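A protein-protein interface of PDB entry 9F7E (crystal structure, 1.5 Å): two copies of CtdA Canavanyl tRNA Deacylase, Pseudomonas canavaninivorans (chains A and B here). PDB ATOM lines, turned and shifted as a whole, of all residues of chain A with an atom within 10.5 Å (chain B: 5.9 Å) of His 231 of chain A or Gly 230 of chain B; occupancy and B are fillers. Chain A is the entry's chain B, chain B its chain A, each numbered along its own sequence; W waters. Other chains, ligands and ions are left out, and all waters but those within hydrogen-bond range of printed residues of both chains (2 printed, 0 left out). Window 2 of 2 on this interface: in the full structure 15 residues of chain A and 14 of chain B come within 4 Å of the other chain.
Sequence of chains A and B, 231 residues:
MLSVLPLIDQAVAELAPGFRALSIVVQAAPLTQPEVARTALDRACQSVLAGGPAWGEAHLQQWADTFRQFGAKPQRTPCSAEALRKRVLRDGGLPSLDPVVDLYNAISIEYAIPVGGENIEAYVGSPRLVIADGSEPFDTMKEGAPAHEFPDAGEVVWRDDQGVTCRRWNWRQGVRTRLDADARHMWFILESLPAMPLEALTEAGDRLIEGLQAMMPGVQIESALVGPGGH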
ATOM      1  N   LEU A   5       8.066 -23.716  -7.648  1.00  0.00           N
ATOM      2  CA  LEU A   5       9.424 -23.289  -7.318  1.00  0.00           C
ATOM      3  C   LEU A   5       9.916 -22.406  -8.454  1.00  0.00           C
ATOM      4  O   LEU A   5      10.487 -22.895  -9.440  1.00  0.00           O
ATOM      5  CB  LEU A   5      10.336 -24.493  -7.086  1.00  0.00           C
ATOM      6  CG  LEU A   5      11.803 -24.174  -6.802  1.00  0.00           C
ATOM      7  CD1 LEU A   5      11.934 -23.179  -5.663  1.00  0.00           C
ATOM      8  CD2 LEU A   5      12.546 -25.482  -6.437  1.00  0.00           C
ATOM      9  N   PRO A   6       9.713 -21.091  -8.361  1.00  0.00           N
ATOM     10  CA  PRO A   6      10.205 -20.226  -9.428  1.00  0.00           C
ATOM     11  C   PRO A   6      11.720 -20.212  -9.415  1.00  0.00           C
ATOM     12  O   PRO A   6      12.357 -20.257  -8.362  1.00  0.00           O
ATOM     13  CB  PRO A   6       9.611 -18.854  -9.098  1.00  0.00           C
ATOM     14  CG  PRO A   6       9.337 -18.895  -7.670  1.00  0.00           C
ATOM     15  CD  PRO A   6       8.979 -20.325  -7.337  1.00  0.00           C
ATOM     16  N   ILE A   8      14.970 -18.003 -10.666  1.00  0.00           N
ATOM     17  CA  ILE A   8      15.435 -16.689 -11.085  1.00  0.00           C
ATOM     18  C   ILE A   8      16.814 -16.904 -11.683  1.00  0.00           C
ATOM     19  O   ILE A   8      17.773 -17.188 -10.961  1.00  0.00           O
ATOM     20  CB  ILE A   8      15.452 -15.694  -9.919  1.00  0.00           C
ATOM     21  CG1 ILE A   8      14.023 -15.587  -9.378  1.00  0.00           C
ATOM     22  CG2 ILE A   8      15.958 -14.359 -10.379  1.00  0.00           C
ATOM     23  CD1 ILE A   8      13.932 -15.281  -7.915  1.00  0.00           C
ATOM     24  N   ALA A  13      19.270 -12.031 -11.819  1.00  0.00           N
ATOM     25  CA  ALA A  13      19.739 -11.638 -10.492  1.00  0.00           C
ATOM     26  C   ALA A  13      20.882 -10.643 -10.580  1.00  0.00           C
ATOM     27  O   ALA A  13      20.967  -9.712  -9.770  1.00  0.00           O
ATOM     28  CB  ALA A  13      20.178 -12.869  -9.706  1.00  0.00           C
ATOM     29  N   ALA A  16      19.233  -7.269 -11.557  1.00  0.00           N
ATOM     30  CA  ALA A  16      18.441  -6.639 -10.500  1.00  0.00           C
ATOM     31  C   ALA A  16      18.790  -7.266  -9.160  1.00  0.00           C
ATOM     32  O   ALA A  16      18.017  -8.052  -8.603  1.00  0.00           O
ATOM     33  CB  ALA A  16      16.938  -6.775 -10.780  1.00  0.00           C
ATOM     34  N   PRO A  17      19.928  -6.899  -8.584  1.00  0.00           N
ATOM     35  CA  PRO A  17      20.401  -7.605  -7.383  1.00  0.00           C
ATOM     36  C   PRO A  17      19.549  -7.404  -6.163  1.00  0.00           C
ATOM     37  O   PRO A  17      19.689  -8.172  -5.208  1.00  0.00           O
ATOM     38  CB  PRO A  17      21.810  -7.019  -7.153  1.00  0.00           C
ATOM     39  CG  PRO A  17      22.132  -6.250  -8.368  1.00  0.00           C
ATOM     40  CD  PRO A  17      20.864  -5.867  -9.053  1.00  0.00           C
ATOM     41  N   GLY A  18      18.678  -6.406  -6.149  1.00  0.00           N
ATOM     42  CA  GLY A  18      17.810  -6.165  -5.032  1.00  0.00           C
ATOM     43  C   GLY A  18      16.430  -6.749  -5.179  1.00  0.00           C
ATOM     44  O   GLY A  18      15.577  -6.494  -4.327  1.00  0.00           O
ATOM     45  N   PHE A  19      16.175  -7.499  -6.240  1.00  0.00           N
ATOM     46  CA  PHE A  19      14.848  -8.053  -6.476  1.00  0.00           C
ATOM     47  C   PHE A  19      14.477  -9.034  -5.375  1.00  0.00           C
ATOM     48  O   PHE A  19      15.231  -9.951  -5.054  1.00  0.00           O
ATOM     49  CB  PHE A  19      14.819  -8.721  -7.852  1.00  0.00           C
ATOM     50  CG  PHE A  19      13.564  -9.460  -8.144  1.00  0.00           C
ATOM     51  CD1 PHE A  19      12.344  -8.806  -8.169  1.00  0.00           C
ATOM     52  CD2 PHE A  19      13.598 -10.811  -8.420  1.00  0.00           C
ATOM     53  CE1 PHE A  19      11.180  -9.492  -8.456  1.00  0.00           C
ATOM     54  CE2 PHE A  19      12.434 -11.517  -8.706  1.00  0.00           C
ATOM     55  CZ  PHE A  19      11.216 -10.843  -8.729  1.00  0.00           C
ATOM     56  N   ARG A  20      13.301  -8.849  -4.808  1.00  0.00           N
ATOM     57  CA  ARG A  20      12.768  -9.827  -3.877  1.00  0.00           C
ATOM     58  C   ARG A  20      11.271  -9.937  -4.103  1.00  0.00           C
ATOM     59  O   ARG A  20      10.611  -8.921  -4.358  1.00  0.00           O
ATOM     60  CB  ARG A  20      13.039  -9.430  -2.436  1.00  0.00           C
ATOM     61  CG  ARG A  20      13.263  -7.988  -2.247  1.00  0.00           C
ATOM     62  CD  ARG A  20      12.957  -7.700  -0.813  1.00  0.00           C
ATOM     63  NE  ARG A  20      13.435  -6.403  -0.369  1.00  0.00           N
ATOM     64  CZ  ARG A  20      12.789  -5.264  -0.550  1.00  0.00           C
ATOM     65  NH1 ARG A  20      11.786  -5.161  -1.405  1.00  0.00           N
ATOM     66  NH2 ARG A  20      13.126  -4.215   0.179  1.00  0.00           N
ATOM     67  N   ALA A  21      10.748 -11.159  -4.033  1.00  0.00           N
ATOM     68  CA  ALA A  21       9.350 -11.387  -4.334  1.00  0.00           C
ATOM     69  C   ALA A  21       8.726 -12.328  -3.320  1.00  0.00           C
ATOM     70  O   ALA A  21       9.385 -13.201  -2.768  1.00  0.00           O
ATOM     71  CB  ALA A  21       9.199 -11.954  -5.744  1.00  0.00           C
ATOM     72  N   SER A 192       9.129  -7.027  -5.974  1.00  0.00           N
ATOM     73  CA  SER A 192       9.588  -5.787  -5.374  1.00  0.00           C
ATOM     74  C   SER A 192      11.071  -5.559  -5.584  1.00  0.00           C
ATOM     75  O   SER A 192      11.856  -6.483  -5.819  1.00  0.00           O
ATOM     76  CB  SER A 192       9.273  -5.760  -3.861  1.00  0.00           C
ATOM     77  OG  SER A 192      10.152  -6.613  -3.159  1.00  0.00           O
ATOM     78  N   LEU A 198      11.017  -4.169   3.012  1.00  0.00           N
ATOM     79  CA  LEU A 198      10.595  -5.550   3.204  1.00  0.00           C
ATOM     80  C   LEU A 198       9.325  -5.652   4.054  1.00  0.00           C
ATOM     81  O   LEU A 198       8.442  -6.482   3.782  1.00  0.00           O
ATOM     82  CB  LEU A 198      11.739  -6.327   3.831  1.00  0.00           C
ATOM     83  CG  LEU A 198      11.467  -7.798   4.076  1.00  0.00           C
ATOM     84  CD1 LEU A 198      11.110  -8.501   2.776  1.00  0.00           C
ATOM     85  CD2 LEU A 198      12.712  -8.356   4.715  1.00  0.00           C
ATOM     86  N   LEU A 201       6.435  -5.165   1.788  1.00  0.00           N
ATOM     87  CA  LEU A 201       6.161  -6.358   0.986  1.00  0.00           C
ATOM     88  C   LEU A 201       5.395  -7.387   1.809  1.00  0.00           C
ATOM     89  O   LEU A 201       4.440  -8.015   1.335  1.00  0.00           O
ATOM     90  CB  LEU A 201       7.468  -6.976   0.477  1.00  0.00           C
ATOM     91  CG  LEU A 201       7.435  -8.315  -0.248  1.00  0.00           C
ATOM     92  CD1 LEU A 201       6.633  -8.234  -1.496  1.00  0.00           C
ATOM     93  CD2 LEU A 201       8.868  -8.770  -0.553  1.00  0.00           C
ATOM     94  N   ALA A 224       6.500 -18.329  -0.261  1.00  0.00           N
ATOM     95  CA  ALA A 224       7.954 -18.316  -0.165  1.00  0.00           C
ATOM     96  C   ALA A 224       8.469 -16.936  -0.530  1.00  0.00           C
ATOM     97  O   ALA A 224       7.952 -16.294  -1.443  1.00  0.00           O
ATOM     98  CB  ALA A 224       8.594 -19.379  -1.077  1.00  0.00           C
ATOM     99  N   LEU A 225       9.493 -16.481   0.184  1.00  0.00           N
ATOM    100  CA  LEU A 225      10.209 -15.259  -0.178  1.00  0.00           C
ATOM    101  C   LEU A 225      11.383 -15.689  -1.049  1.00  0.00           C
ATOM    102  O   LEU A 225      12.184 -16.550  -0.642  1.00  0.00           O
ATOM    103  CB  LEU A 225      10.665 -14.546   1.090  1.00  0.00           C
ATOM    104  CG  LEU A 225      11.257 -13.152   0.951  1.00  0.00           C
ATOM    105  CD1 LEU A 225      10.182 -12.127   0.602  1.00  0.00           C
ATOM    106  CD2 LEU A 225      11.989 -12.786   2.248  1.00  0.00           C
ATOM    107  N   VAL A 226      11.458 -15.141  -2.258  1.00  0.00           N
ATOM    108  CA  VAL A 226      12.463 -15.538  -3.229  1.00  0.00           C
ATOM    109  C   VAL A 226      13.171 -14.312  -3.813  1.00  0.00           C
ATOM    110  O   VAL A 226      12.688 -13.173  -3.742  1.00  0.00           O
ATOM    111  CB  VAL A 226      11.825 -16.388  -4.354  1.00  0.00           C
ATOM    112  CG1 VAL A 226      11.082 -17.578  -3.770  1.00  0.00           C
ATOM    113  CG2 VAL A 226      10.903 -15.547  -5.202  1.00  0.00           C
ATOM    114  N   GLY A 227      14.323 -14.568  -4.439  1.00  0.00           N
ATOM    115  CA  GLY A 227      15.055 -13.552  -5.158  1.00  0.00           C
ATOM    116  C   GLY A 227      16.376 -13.168  -4.528  1.00  0.00           C
ATOM    117  O   GLY A 227      16.622 -13.434  -3.350  1.00  0.00           O
ATOM    118  N   PRO A 228      17.243 -12.494  -5.295  1.00  0.00           N
ATOM    119  CA  PRO A 228      18.571 -12.133  -4.755  1.00  0.00           C
ATOM    120  C   PRO A 228      18.525 -11.149  -3.604  1.00  0.00           C
ATOM    121  O   PRO A 228      19.465 -11.128  -2.802  1.00  0.00           O
ATOM    122  CB  PRO A 228      19.299 -11.518  -5.966  1.00  0.00           C
ATOM    123  CG  PRO A 228      18.200 -11.077  -6.885  1.00  0.00           C
ATOM    124  CD  PRO A 228      17.081 -12.084  -6.702  1.00  0.00           C
ATOM    125  N   GLY A 229      17.472 -10.350  -3.486  1.00  0.00           N
ATOM    126  CA  GLY A 229      17.334  -9.408  -2.400  1.00  0.00           C
ATOM    127  C   GLY A 229      16.586  -9.911  -1.195  1.00  0.00           C
ATOM    128  O   GLY A 229      16.249  -9.109  -0.322  1.00  0.00           O
ATOM    129  N   GLY A 230      16.324 -11.214  -1.116  1.00  0.00           N
ATOM    130  CA  GLY A 230      15.400 -11.776  -0.140  1.00  0.00           C
ATOM    131  C   GLY A 230      16.086 -12.541   0.979  1.00  0.00           C
ATOM    132  O   GLY A 230      15.402 -13.210   1.767  1.00  0.00           O
ATOM    133  N   HIS A 231      17.408 -12.477   1.067  1.00  0.00           N
ATOM    134  CA  HIS A 231      18.130 -13.327   2.002  1.00  0.00           C
ATOM    135  C   HIS A 231      18.758 -12.507   3.123  1.00  0.00           C
ATOM    136  O   HIS A 231      19.493 -13.044   3.955  1.00  0.00           O
ATOM    137  CB  HIS A 231      19.198 -14.146   1.256  1.00  0.00           C
ATOM    138  CG  HIS A 231      18.671 -14.870   0.052  1.00  0.00           C
ATOM    139  ND1 HIS A 231      17.726 -15.869   0.143  1.00  0.00           N
ATOM    140  CD2 HIS A 231      18.955 -14.742  -1.265  1.00  0.00           C
ATOM    141  CE1 HIS A 231      17.443 -16.319  -1.065  1.00  0.00           C
ATOM    142  NE2 HIS A 231      18.181 -15.656  -1.938  1.00  0.00           N
ATOM    143  OXT HIS A 231      18.532 -11.298   3.228  1.00  0.00           O
ATOM    144  N   ILE B   8      20.237 -12.474  11.400  1.00  0.00           N
ATOM    145  CA  ILE B   8      21.550 -13.066  11.585  1.00  0.00           C
ATOM    146  C   ILE B   8      22.529 -11.932  11.758  1.00  0.00           C
ATOM    147  O   ILE B   8      22.749 -11.145  10.828  1.00  0.00           O
ATOM    148  CB  ILE B   8      21.936 -13.970  10.417  1.00  0.00           C
ATOM    149  CG1 ILE B   8      20.905 -15.092  10.315  1.00  0.00           C
ATOM    150  CG2 ILE B   8      23.337 -14.505  10.608  1.00  0.00           C
ATOM    151  CD1 ILE B   8      20.725 -15.614   8.972  1.00  0.00           C
ATOM    152  N   GLY B  18      29.435 -19.431   4.930  1.00  0.00           N
ATOM    153  CA  GLY B  18      28.672 -20.340   4.106  1.00  0.00           C
ATOM    154  C   GLY B  18      27.371 -20.804   4.711  1.00  0.00           C
ATOM    155  O   GLY B  18      26.699 -21.670   4.137  1.00  0.00           O
ATOM    156  N   PHE B  19      27.008 -20.280   5.865  1.00  0.00           N
ATOM    157  CA  PHE B  19      25.754 -20.658   6.507  1.00  0.00           C
ATOM    158  C   PHE B  19      24.546 -20.238   5.688  1.00  0.00           C
ATOM    159  O   PHE B  19      24.413 -19.083   5.283  1.00  0.00           O
ATOM    160  CB  PHE B  19      25.694 -20.006   7.895  1.00  0.00           C
ATOM    161  CG  PHE B  19      24.381 -20.177   8.603  1.00  0.00           C
ATOM    162  CD1 PHE B  19      23.919 -21.429   8.940  1.00  0.00           C
ATOM    163  CD2 PHE B  19      23.667 -19.075   9.003  1.00  0.00           C
ATOM    164  CE1 PHE B  19      22.717 -21.563   9.635  1.00  0.00           C
ATOM    165  CE2 PHE B  19      22.489 -19.189   9.687  1.00  0.00           C
ATOM    166  CZ  PHE B  19      21.992 -20.448  10.007  1.00  0.00           C
ATOM    167  N   ARG B  20      23.616 -21.191   5.501  1.00  0.00           N
ATOM    168  CA  ARG B  20      22.398 -20.999   4.731  1.00  0.00           C
ATOM    169  C   ARG B  20      21.321 -21.778   5.463  1.00  0.00           C
ATOM    170  O   ARG B  20      21.555 -22.920   5.826  1.00  0.00           O
ATOM    171  CB  ARG B  20      22.626 -21.490   3.287  1.00  0.00           C
ATOM    172  CG  ARG B  20      21.423 -21.676   2.430  1.00  0.00           C
ATOM    173  CD  ARG B  20      21.837 -21.704   0.960  1.00  0.00           C
ATOM    174  NE  ARG B  20      22.682 -22.842   0.612  1.00  0.00           N
ATOM    175  CZ  ARG B  20      23.365 -22.949  -0.520  1.00  0.00           C
ATOM    176  NH1 ARG B  20      23.383 -21.973  -1.412  1.00  0.00           N
ATOM    177  NH2 ARG B  20      24.054 -24.062  -0.759  1.00  0.00           N
ATOM    178  N   LEU B 225      14.734 -18.484   2.709  1.00  0.00           N
ATOM    179  CA  LEU B 225      16.129 -18.880   2.818  1.00  0.00           C
ATOM    180  C   LEU B 225      16.942 -17.703   3.326  1.00  0.00           C
ATOM    181  O   LEU B 225      16.889 -16.624   2.743  1.00  0.00           O
ATOM    182  CB  LEU B 225      16.618 -19.341   1.453  1.00  0.00           C
ATOM    183  CG  LEU B 225      18.007 -19.962   1.308  1.00  0.00           C
ATOM    184  CD1 LEU B 225      17.937 -21.324   1.928  1.00  0.00           C
ATOM    185  CD2 LEU B 225      18.429 -19.964  -0.148  1.00  0.00           C
ATOM    186  N   VAL B 226      17.687 -17.913   4.400  1.00  0.00           N
ATOM    187  CA  VAL B 226      18.441 -16.844   5.034  1.00  0.00           C
ATOM    188  C   VAL B 226      19.901 -17.251   5.217  1.00  0.00           C
ATOM    189  O   VAL B 226      20.266 -18.428   5.175  1.00  0.00           O
ATOM    190  CB  VAL B 226      17.830 -16.420   6.407  1.00  0.00           C
ATOM    191  CG1 VAL B 226      16.393 -15.953   6.244  1.00  0.00           C
ATOM    192  CG2 VAL B 226      17.957 -17.532   7.459  1.00  0.00           C
ATOM    193  N   GLY B 227      20.737 -16.245   5.468  1.00  0.00           N
ATOM    194  CA  GLY B 227      22.124 -16.479   5.793  1.00  0.00           C
ATOM    195  C   GLY B 227      23.067 -15.989   4.711  1.00  0.00           C
ATOM    196  O   GLY B 227      22.689 -15.764   3.564  1.00  0.00           O
ATOM    197  N   PRO B 228      24.337 -15.847   5.072  1.00  0.00           N
ATOM    198  CA  PRO B 228      25.331 -15.345   4.101  1.00  0.00           C
ATOM    199  C   PRO B 228      25.603 -16.308   2.978  1.00  0.00           C
ATOM    200  O   PRO B 228      26.134 -15.889   1.938  1.00  0.00           O
ATOM    201  CB  PRO B 228      26.573 -15.099   4.964  1.00  0.00           C
ATOM    202  CG  PRO B 228      26.405 -15.984   6.137  1.00  0.00           C
ATOM    203  CD  PRO B 228      24.912 -16.074   6.411  1.00  0.00           C
ATOM    204  N   GLY B 229      25.321 -17.598   3.160  1.00  0.00           N
ATOM    205  CA  GLY B 229      25.528 -18.525   2.089  1.00  0.00           C
ATOM    206  C   GLY B 229      24.345 -18.693   1.189  1.00  0.00           C
ATOM    207  O   GLY B 229      24.422 -19.510   0.266  1.00  0.00           O
ATOM    208  N   GLY B 230      23.265 -17.953   1.409  1.00  0.00           N
ATOM    209  CA  GLY B 230      22.149 -17.950   0.471  1.00  0.00           C
ATOM    210  C   GLY B 230      22.321 -16.812  -0.525  1.00  0.00           C
ATOM    211  O   GLY B 230      22.663 -15.688  -0.149  1.00  0.00           O
ATOM    212  N   HIS B 231      22.101 -17.125  -1.803  1.00  0.00           N
ATOM    213  CA  HIS B 231      22.271 -16.150  -2.889  1.00  0.00           C
ATOM    214  C   HIS B 231      21.212 -16.362  -3.978  1.00  0.00           C
ATOM    215  O   HIS B 231      20.138 -15.760  -3.961  1.00  0.00           O
ATOM    216  CB  HIS B 231      23.666 -16.265  -3.513  1.00  0.00           C
ATOM    217  CG  HIS B 231      24.778 -16.271  -2.513  1.00  0.00           C
ATOM    218  ND1 HIS B 231      25.069 -15.188  -1.711  1.00  0.00           N
ATOM    219  CD2 HIS B 231      25.660 -17.241  -2.169  1.00  0.00           C
ATOM    220  CE1 HIS B 231      26.087 -15.486  -0.923  1.00  0.00           C
ATOM    221  NE2 HIS B 231      26.466 -16.726  -1.184  1.00  0.00           N
HETATM  222  O   HOH W   1      14.401 -16.192   0.778  1.00  0.00           O
HETATM  223  O   HOH W   2      20.574 -13.408   6.198  1.00  0.00           O
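Water W2 lies within hydrogen-bond range of O of His 231 of chain A and N of Gly 227 of chain B. Water W1 lies within hydrogen-bond range of O of Leu 225 of chain A, N of Leu 225 of chain B, O of Gly 230 of chain A and ND1 of His 231 of chain A.
Hydrophobic or aromatic side chains of chain B that line the printed part of chain A: Leu 225. Along chain B the printed residues that touch a printed residue of chain A span positions 225 to 231. Of the 21 printed residues of chain A, 2 touch a printed residue of chain B. Printed residues of chain A that touch a printed residue of chain B: Gly 230 and His 231. Hydrophobic or aromatic side chains of chain A within 4 Å of the printed part of chain B: His 231.
Among the printed residues, merely in contact across the chains: His 231 of chain A with Gly 227 of chain B (3.8 Å), Gly 230 of chain A with Leu 225 of chain B (3.8 Å) and His 231 of chain A with Gly 230 of chain B (3.99 Å).
NE2 of His 231 of chain B sits close to O of Pro 228 of chain B (3.2 Å). O of Gly 227 of chain A sits at hydrogen-bond distance from NE2 of His 231 of chain A (3.1 Å).
ND1 of His 231 of chain A is in hydrogen-bond range of O of Leu 225 of chain B, 2.8 Å away. A ring nitrogen (NE2) of His 231 of chain A is in hydrogen-bond range of the backbone carbonyl oxygen (O) of His 231 of chain B (2.8 Å).
His 231 of chain A touches Leu 225 of chain B, but with the chains exchanged Leu 225 of chain A does not touch His 231 of chain B (8.7 Å). His 231 of chain A touches Gly 227 of chain B, but with the chains exchanged Gly 227 of chain A does not touch His 231 of chain B (4.3 Å). His 231 of chain A touches Gly 230 of chain B, but with the chains exchanged Gly 230 of chain A does not touch His 231 of chain B (6.6 Å). His 231 of chain B touches its own counterpart, His 231 of chain A. Positions printed for both chains: 8, 18, 19, 20, 225, 226, 227, 228, 229, 230 and 231. Of the 5 pairs that touch across the chains among the printed residues, 1 has its exchanged pair printed and touching as well.
Of the printed residues of chain B, Gly 230 of chain A touches Leu 225. Of the printed residues of chain B, His 231 of chain A touches Leu 225, Gly 227, Gly 230 and His 231. Leu 225 of chain B touches just these residues of chain A: Gly 230 (3.8 Å) and His 231 (2.8 Å). No residue of chain A comes within 4 Å of Val 226 of chain B. No residue of chain A comes within 4 Å of Pro 228 of chain B. Of the printed residues of chain A, Gly 230 of chain B touches His 231. His 231 of chain B touches one residue of chain A. The nearest printed residue of chain A that does not touch Gly 230 of chain B is Pro 228 of chain A (6.2 Å). The nearest printed residue of chain B that does not touch Gly 230 of chain A is Val 226 of chain B (5.3 Å).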
